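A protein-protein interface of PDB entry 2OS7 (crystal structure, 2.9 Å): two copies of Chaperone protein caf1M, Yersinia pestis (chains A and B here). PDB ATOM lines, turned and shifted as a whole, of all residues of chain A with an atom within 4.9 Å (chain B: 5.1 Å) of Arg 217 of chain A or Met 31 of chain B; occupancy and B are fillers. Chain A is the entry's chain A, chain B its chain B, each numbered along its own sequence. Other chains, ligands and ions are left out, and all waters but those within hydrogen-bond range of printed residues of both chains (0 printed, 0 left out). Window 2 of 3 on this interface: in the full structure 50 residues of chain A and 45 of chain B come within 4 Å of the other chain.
OG of Ser 33 of chain B lies within hydrogen-bond range of O of Gly 180 of chain A. OG of Ser 77 of chain B sits at hydrogen-bond distance from OE2 of Glu 181 of chain A (2.8 Å). N of Leu 225 of chain A lies within hydrogen-bond range of O of Met 31 of chain B (2.9 Å).
The backbone NH (N) of Gly 180 of chain A is in hydrogen-bond range of the backbone carbonyl oxygen (O) of Arg 217 of chain A (2.8 Å). The side-chain sulfur (SD) of Met 31 of chain B sits at hydrogen-bond distance from the guanidinium group (NE) of Arg 79 of chain B, at 3.7 Å. The guanidinium group of Arg 217 of chain A is in hydrogen-bond range of the backbone carbonyl oxygen of Asp 226 of chain A (2.7 Å). O of Val 32 of chain B is in hydrogen-bond range of N of Leu 78 of chain B (2.7 Å). The side-chain carboxylate (OE2) of Glu 181 of chain A lies within salt-bridge range of the guanidinium group (NE) of Arg 217 of chain A, at 3.0 Å.
Among the printed residues, merely in contact across the chains: Arg 217 of chain A with Met 31 of chain B, Gly 224 of chain A with Met 31 of chain B, Leu 225 of chain A with Val 32 of chain B, Leu 225 of chain A with Ser 33 of chain B and Leu 225 of chain A with Ser 77 of chain B.
Of chain B, only Met 31 comes within 4 Å of Arg 217 of chain A. Met 31 of chain B touches just these residues of chain A: Arg 217, Gly 224 and Leu 225. Of the printed residues of chain B, Gly 224 of chain A touches Met 31. Of the printed residues of chain B, Leu 225 of chain A touches Met 31, Val 32, Ser 33 and Ser 77. Printed residues of chain A within 4 Å of Ser 33 of chain B: Gly 180 (2.8 Å) and Leu 225 (3.3 Å). Ile 218 of chain A touches none of the printed residues of chain B. The nearest printed residue of chain B that does not touch Gly 224 of chain A is Val 32 of chain B (4.9 Å).
Of the 8 printed residues of chain B, 4 touch a printed residue of chain A. Hydrophobic or aromatic side chains of chain B within 4 Å of the printed part of chain A: Met 31. Printed residues of chain A that touch a printed residue of chain B: Gly 180, Glu 181, Arg 217, Gly 224 and Leu 225. Hydrophobic or aromatic side chains of chain A that line the printed part of chain B: Leu 225.
No position is printed for both chains.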
ATOM      1  N   ASN A 178     -20.310  32.740 -23.024  1.00  0.00           N
ATOM      2  CA  ASN A 178     -18.882  32.545 -23.187  1.00  0.00           C
ATOM      3  C   ASN A 178     -18.643  31.185 -23.865  1.00  0.00           C
ATOM      4  O   ASN A 178     -18.537  30.141 -23.212  1.00  0.00           O
ATOM      5  CB  ASN A 178     -18.144  32.693 -21.850  1.00  0.00           C
ATOM      6  CG  ASN A 178     -18.226  34.147 -21.265  1.00  0.00           C
ATOM      7  OD1 ASN A 178     -18.638  34.336 -20.116  1.00  0.00           O
ATOM      8  ND2 ASN A 178     -17.818  35.165 -22.051  1.00  0.00           N
ATOM      9  N   ILE A 179     -18.610  31.225 -25.196  1.00  0.00           N
ATOM     10  CA  ILE A 179     -18.507  30.057 -26.066  1.00  0.00           C
ATOM     11  C   ILE A 179     -17.098  29.496 -26.009  1.00  0.00           C
ATOM     12  O   ILE A 179     -16.137  30.248 -26.036  1.00  0.00           O
ATOM     13  CB  ILE A 179     -18.926  30.435 -27.512  1.00  0.00           C
ATOM     14  CG1 ILE A 179     -20.429  30.223 -27.664  1.00  0.00           C
ATOM     15  CG2 ILE A 179     -18.158  29.646 -28.543  1.00  0.00           C
ATOM     16  CD1 ILE A 179     -20.980  30.678 -28.987  1.00  0.00           C
ATOM     17  N   GLY A 180     -16.985  28.181 -25.909  1.00  0.00           N
ATOM     18  CA  GLY A 180     -15.693  27.525 -25.839  1.00  0.00           C
ATOM     19  C   GLY A 180     -15.527  26.441 -26.895  1.00  0.00           C
ATOM     20  O   GLY A 180     -14.460  25.866 -27.052  1.00  0.00           O
ATOM     21  N   GLU A 181     -16.588  26.153 -27.635  1.00  0.00           N
ATOM     22  CA  GLU A 181     -16.460  25.228 -28.735  1.00  0.00           C
ATOM     23  C   GLU A 181     -17.407  25.589 -29.843  1.00  0.00           C
ATOM     24  O   GLU A 181     -18.601  25.611 -29.672  1.00  0.00           O
ATOM     25  CB  GLU A 181     -16.750  23.811 -28.278  1.00  0.00           C
ATOM     26  CG  GLU A 181     -15.923  22.793 -28.996  1.00  0.00           C
ATOM     27  CD  GLU A 181     -16.681  21.541 -29.245  1.00  0.00           C
ATOM     28  OE1 GLU A 181     -17.511  21.549 -30.190  1.00  0.00           O
ATOM     29  OE2 GLU A 181     -16.445  20.551 -28.507  1.00  0.00           O
ATOM     30  N   SER A 215     -22.485  23.858 -34.434  1.00  0.00           N
ATOM     31  CA  SER A 215     -22.367  23.125 -33.182  1.00  0.00           C
ATOM     32  C   SER A 215     -21.571  23.923 -32.155  1.00  0.00           C
ATOM     33  O   SER A 215     -20.563  24.550 -32.511  1.00  0.00           O
ATOM     34  CB  SER A 215     -21.668  21.812 -33.448  1.00  0.00           C
ATOM     35  OG  SER A 215     -22.276  20.792 -32.699  1.00  0.00           O
ATOM     36  N   TRP A 216     -21.989  23.908 -30.890  1.00  0.00           N
ATOM     37  CA  TRP A 216     -21.364  24.775 -29.890  1.00  0.00           C
ATOM     38  C   TRP A 216     -21.440  24.252 -28.452  1.00  0.00           C
ATOM     39  O   TRP A 216     -22.276  23.423 -28.095  1.00  0.00           O
ATOM     40  CB  TRP A 216     -21.929  26.213 -29.974  1.00  0.00           C
ATOM     41  CG  TRP A 216     -23.331  26.403 -29.362  1.00  0.00           C
ATOM     42  CD1 TRP A 216     -23.622  26.692 -28.060  1.00  0.00           C
ATOM     43  CD2 TRP A 216     -24.602  26.296 -30.036  1.00  0.00           C
ATOM     44  NE1 TRP A 216     -24.984  26.778 -27.883  1.00  0.00           N
ATOM     45  CE2 TRP A 216     -25.607  26.534 -29.078  1.00  0.00           C
ATOM     46  CE3 TRP A 216     -24.989  26.011 -31.357  1.00  0.00           C
ATOM     47  CZ2 TRP A 216     -26.983  26.507 -29.406  1.00  0.00           C
ATOM     48  CZ3 TRP A 216     -26.360  25.967 -31.671  1.00  0.00           C
ATOM     49  CH2 TRP A 216     -27.328  26.223 -30.701  1.00  0.00           C
ATOM     50  N   ARG A 217     -20.531  24.755 -27.636  1.00  0.00           N
ATOM     51  CA  ARG A 217     -20.531  24.548 -26.200  1.00  0.00           C
ATOM     52  C   ARG A 217     -20.155  25.862 -25.531  1.00  0.00           C
ATOM     53  O   ARG A 217     -19.259  26.569 -26.000  1.00  0.00           O
ATOM     54  CB  ARG A 217     -19.513  23.488 -25.803  1.00  0.00           C
ATOM     55  CG  ARG A 217     -19.801  22.122 -26.348  1.00  0.00           C
ATOM     56  CD  ARG A 217     -18.576  21.279 -26.205  1.00  0.00           C
ATOM     57  NE  ARG A 217     -18.768  19.922 -26.704  1.00  0.00           N
ATOM     58  CZ  ARG A 217     -19.152  18.893 -25.950  1.00  0.00           C
ATOM     59  NH1 ARG A 217     -19.385  19.060 -24.645  1.00  0.00           N
ATOM     60  NH2 ARG A 217     -19.296  17.692 -26.503  1.00  0.00           N
ATOM     61  N   ILE A 218     -20.855  26.206 -24.457  1.00  0.00           N
ATOM     62  CA  ILE A 218     -20.406  27.315 -23.658  1.00  0.00           C
ATOM     63  C   ILE A 218     -19.502  26.815 -22.511  1.00  0.00           C
ATOM     64  O   ILE A 218     -19.352  25.603 -22.300  1.00  0.00           O
ATOM     65  CB  ILE A 218     -21.578  28.224 -23.195  1.00  0.00           C
ATOM     66  CG1 ILE A 218     -22.364  27.626 -22.032  1.00  0.00           C
ATOM     67  CG2 ILE A 218     -22.492  28.549 -24.368  1.00  0.00           C
ATOM     68  CD1 ILE A 218     -23.321  28.614 -21.404  1.00  0.00           C
ATOM     69  N   ILE A 219     -18.873  27.748 -21.799  1.00  0.00           N
ATOM     70  CA  ILE A 219     -18.048  27.402 -20.654  1.00  0.00           C
ATOM     71  C   ILE A 219     -18.834  27.567 -19.352  1.00  0.00           C
ATOM     72  O   ILE A 219     -19.292  28.659 -19.024  1.00  0.00           O
ATOM     73  CB  ILE A 219     -16.756  28.231 -20.607  1.00  0.00           C
ATOM     74  CG1 ILE A 219     -15.945  28.031 -21.896  1.00  0.00           C
ATOM     75  CG2 ILE A 219     -15.915  27.777 -19.446  1.00  0.00           C
ATOM     76  CD1 ILE A 219     -14.614  28.845 -22.026  1.00  0.00           C
ATOM     77  N   GLY A 224     -15.427  24.012 -16.934  1.00  0.00           N
ATOM     78  CA  GLY A 224     -15.551  23.030 -17.990  1.00  0.00           C
ATOM     79  C   GLY A 224     -16.445  23.470 -19.137  1.00  0.00           C
ATOM     80  O   GLY A 224     -16.991  24.570 -19.144  1.00  0.00           O
ATOM     81  N   LEU A 225     -16.565  22.605 -20.131  1.00  0.00           N
ATOM     82  CA  LEU A 225     -17.407  22.857 -21.254  1.00  0.00           C
ATOM     83  C   LEU A 225     -18.732  22.179 -21.003  1.00  0.00           C
ATOM     84  O   LEU A 225     -18.814  21.038 -20.490  1.00  0.00           O
ATOM     85  CB  LEU A 225     -16.772  22.307 -22.522  1.00  0.00           C
ATOM     86  CG  LEU A 225     -15.579  23.059 -23.091  1.00  0.00           C
ATOM     87  CD1 LEU A 225     -14.875  22.174 -24.065  1.00  0.00           C
ATOM     88  CD2 LEU A 225     -16.037  24.321 -23.766  1.00  0.00           C
ATOM     89  N   ASP A 226     -19.778  22.900 -21.387  1.00  0.00           N
ATOM     90  CA  ASP A 226     -21.159  22.429 -21.355  1.00  0.00           C
ATOM     91  C   ASP A 226     -21.436  21.343 -22.398  1.00  0.00           C
ATOM     92  O   ASP A 226     -20.565  20.890 -23.125  1.00  0.00           O
ATOM     93  CB  ASP A 226     -22.057  23.641 -21.614  1.00  0.00           C
ATOM     94  CG  ASP A 226     -23.444  23.484 -21.042  1.00  0.00           C
ATOM     95  OD1 ASP A 226     -23.650  22.571 -20.212  1.00  0.00           O
ATOM     96  OD2 ASP A 226     -24.328  24.287 -21.426  1.00  0.00           O
ATOM     97  N   ARG A 227     -22.678  20.929 -22.478  1.00  0.00           N
ATOM     98  CA  ARG A 227     -23.048  19.949 -23.476  1.00  0.00           C
ATOM     99  C   ARG A 227     -22.980  20.540 -24.896  1.00  0.00           C
ATOM    100  O   ARG A 227     -23.015  21.748 -25.065  1.00  0.00           O
ATOM    101  CB  ARG A 227     -24.421  19.359 -23.148  1.00  0.00           C
ATOM    102  CG  ARG A 227     -25.500  20.369 -22.869  1.00  0.00           C
ATOM    103  CD  ARG A 227     -26.869  19.783 -23.258  1.00  0.00           C
ATOM    104  NE  ARG A 227     -26.880  19.401 -24.686  1.00  0.00           N
ATOM    105  CZ  ARG A 227     -27.837  18.710 -25.294  1.00  0.00           C
ATOM    106  NH1 ARG A 227     -28.909  18.326 -24.613  1.00  0.00           N
ATOM    107  NH2 ARG A 227     -27.723  18.438 -26.594  1.00  0.00           N
ATOM    108  N   LEU A 228     -22.836  19.676 -25.891  1.00  0.00           N
ATOM    109  CA  LEU A 228     -22.965  20.056 -27.294  1.00  0.00           C
ATOM    110  C   LEU A 228     -24.412  20.345 -27.688  1.00  0.00           C
ATOM    111  O   LEU A 228     -25.339  19.665 -27.275  1.00  0.00           O
ATOM    112  CB  LEU A 228     -22.413  18.944 -28.195  1.00  0.00           C
ATOM    113  CG  LEU A 228     -21.942  19.345 -29.589  1.00  0.00           C
ATOM    114  CD1 LEU A 228     -20.580  20.091 -29.576  1.00  0.00           C
ATOM    115  CD2 LEU A 228     -21.884  18.143 -30.498  1.00  0.00           C
ATOM    116  N   GLY B  29     -16.628  11.610 -17.423  1.00  0.00           N
ATOM    117  CA  GLY B  29     -15.563  12.565 -17.624  1.00  0.00           C
ATOM    118  C   GLY B  29     -15.952  14.031 -17.614  1.00  0.00           C
ATOM    119  O   GLY B  29     -17.101  14.387 -17.342  1.00  0.00           O
ATOM    120  N   VAL B  30     -14.973  14.883 -17.887  1.00  0.00           N
ATOM    121  CA  VAL B  30     -15.225  16.301 -18.095  1.00  0.00           C
ATOM    122  C   VAL B  30     -14.586  16.806 -19.405  1.00  0.00           C
ATOM    123  O   VAL B  30     -13.649  16.219 -19.921  1.00  0.00           O
ATOM    124  CB  VAL B  30     -14.755  17.159 -16.894  1.00  0.00           C
ATOM    125  CG1 VAL B  30     -15.511  16.787 -15.650  1.00  0.00           C
ATOM    126  CG2 VAL B  30     -13.256  17.007 -16.672  1.00  0.00           C
ATOM    127  N   MET B  31     -15.124  17.890 -19.937  1.00  0.00           N
ATOM    128  CA  MET B  31     -14.577  18.525 -21.128  1.00  0.00           C
ATOM    129  C   MET B  31     -13.965  19.883 -20.761  1.00  0.00           C
ATOM    130  O   MET B  31     -14.521  20.624 -19.947  1.00  0.00           O
ATOM    131  CB  MET B  31     -15.675  18.745 -22.171  1.00  0.00           C
ATOM    132  CG  MET B  31     -16.494  17.528 -22.506  1.00  0.00           C
ATOM    133  SD  MET B  31     -15.761  16.629 -23.853  1.00  0.00           S
ATOM    134  CE  MET B  31     -16.418  17.550 -25.235  1.00  0.00           C
ATOM    135  N   VAL B  32     -12.826  20.196 -21.379  1.00  0.00           N
ATOM    136  CA  VAL B  32     -12.084  21.414 -21.100  1.00  0.00           C
ATOM    137  C   VAL B  32     -11.624  22.047 -22.399  1.00  0.00           C
ATOM    138  O   VAL B  32     -11.129  21.349 -23.271  1.00  0.00           O
ATOM    139  CB  VAL B  32     -10.855  21.111 -20.275  1.00  0.00           C
ATOM    140  CG1 VAL B  32     -10.043  22.362 -20.103  1.00  0.00           C
ATOM    141  CG2 VAL B  32     -11.262  20.566 -18.915  1.00  0.00           C
ATOM    142  N   SER B  33     -11.798  23.361 -22.518  1.00  0.00           N
ATOM    143  CA  SER B  33     -11.343  24.103 -23.674  1.00  0.00           C
ATOM    144  C   SER B  33      -9.874  24.345 -23.603  1.00  0.00           C
ATOM    145  O   SER B  33      -9.347  24.586 -22.522  1.00  0.00           O
ATOM    146  CB  SER B  33     -12.001  25.451 -23.739  1.00  0.00           C
ATOM    147  OG  SER B  33     -13.023  25.382 -24.677  1.00  0.00           O
ATOM    148  N   SER B  77     -11.497  20.811 -27.580  1.00  0.00           N
ATOM    149  CA  SER B  77     -11.825  20.280 -26.244  1.00  0.00           C
ATOM    150  C   SER B  77     -10.830  19.214 -25.818  1.00  0.00           C
ATOM    151  O   SER B  77     -10.191  18.614 -26.660  1.00  0.00           O
ATOM    152  CB  SER B  77     -13.218  19.680 -26.248  1.00  0.00           C
ATOM    153  OG  SER B  77     -14.118  20.516 -26.940  1.00  0.00           O
ATOM    154  N   LEU B  78     -10.677  18.988 -24.520  1.00  0.00           N
ATOM    155  CA  LEU B  78      -9.966  17.796 -24.021  1.00  0.00           C
ATOM    156  C   LEU B  78     -10.905  17.022 -23.123  1.00  0.00           C
ATOM    157  O   LEU B  78     -11.684  17.623 -22.394  1.00  0.00           O
ATOM    158  CB  LEU B  78      -8.757  18.161 -23.181  1.00  0.00           C
ATOM    159  CG  LEU B  78      -7.539  18.903 -23.696  1.00  0.00           C
ATOM    160  CD1 LEU B  78      -6.594  19.215 -22.535  1.00  0.00           C
ATOM    161  CD2 LEU B  78      -6.831  18.116 -24.776  1.00  0.00           C
ATOM    162  N   ARG B  79     -10.834  15.703 -23.146  1.00  0.00           N
ATOM    163  CA  ARG B  79     -11.645  14.935 -22.229  1.00  0.00           C
ATOM    164  C   ARG B  79     -10.756  14.363 -21.117  1.00  0.00           C
ATOM    165  O   ARG B  79      -9.842  13.570 -21.358  1.00  0.00           O
ATOM    166  CB  ARG B  79     -12.519  13.897 -22.965  1.00  0.00           C
ATOM    167  CG  ARG B  79     -13.211  12.866 -22.070  1.00  0.00           C
ATOM    168  CD  ARG B  79     -14.557  12.316 -22.627  1.00  0.00           C
ATOM    169  NE  ARG B  79     -15.654  13.249 -22.294  1.00  0.00           N
ATOM    170  CZ  ARG B  79     -16.653  13.037 -21.415  1.00  0.00           C
ATOM    171  NH1 ARG B  79     -16.768  11.876 -20.773  1.00  0.00           N
ATOM    172  NH2 ARG B  79     -17.560  13.994 -21.189  1.00  0.00           N
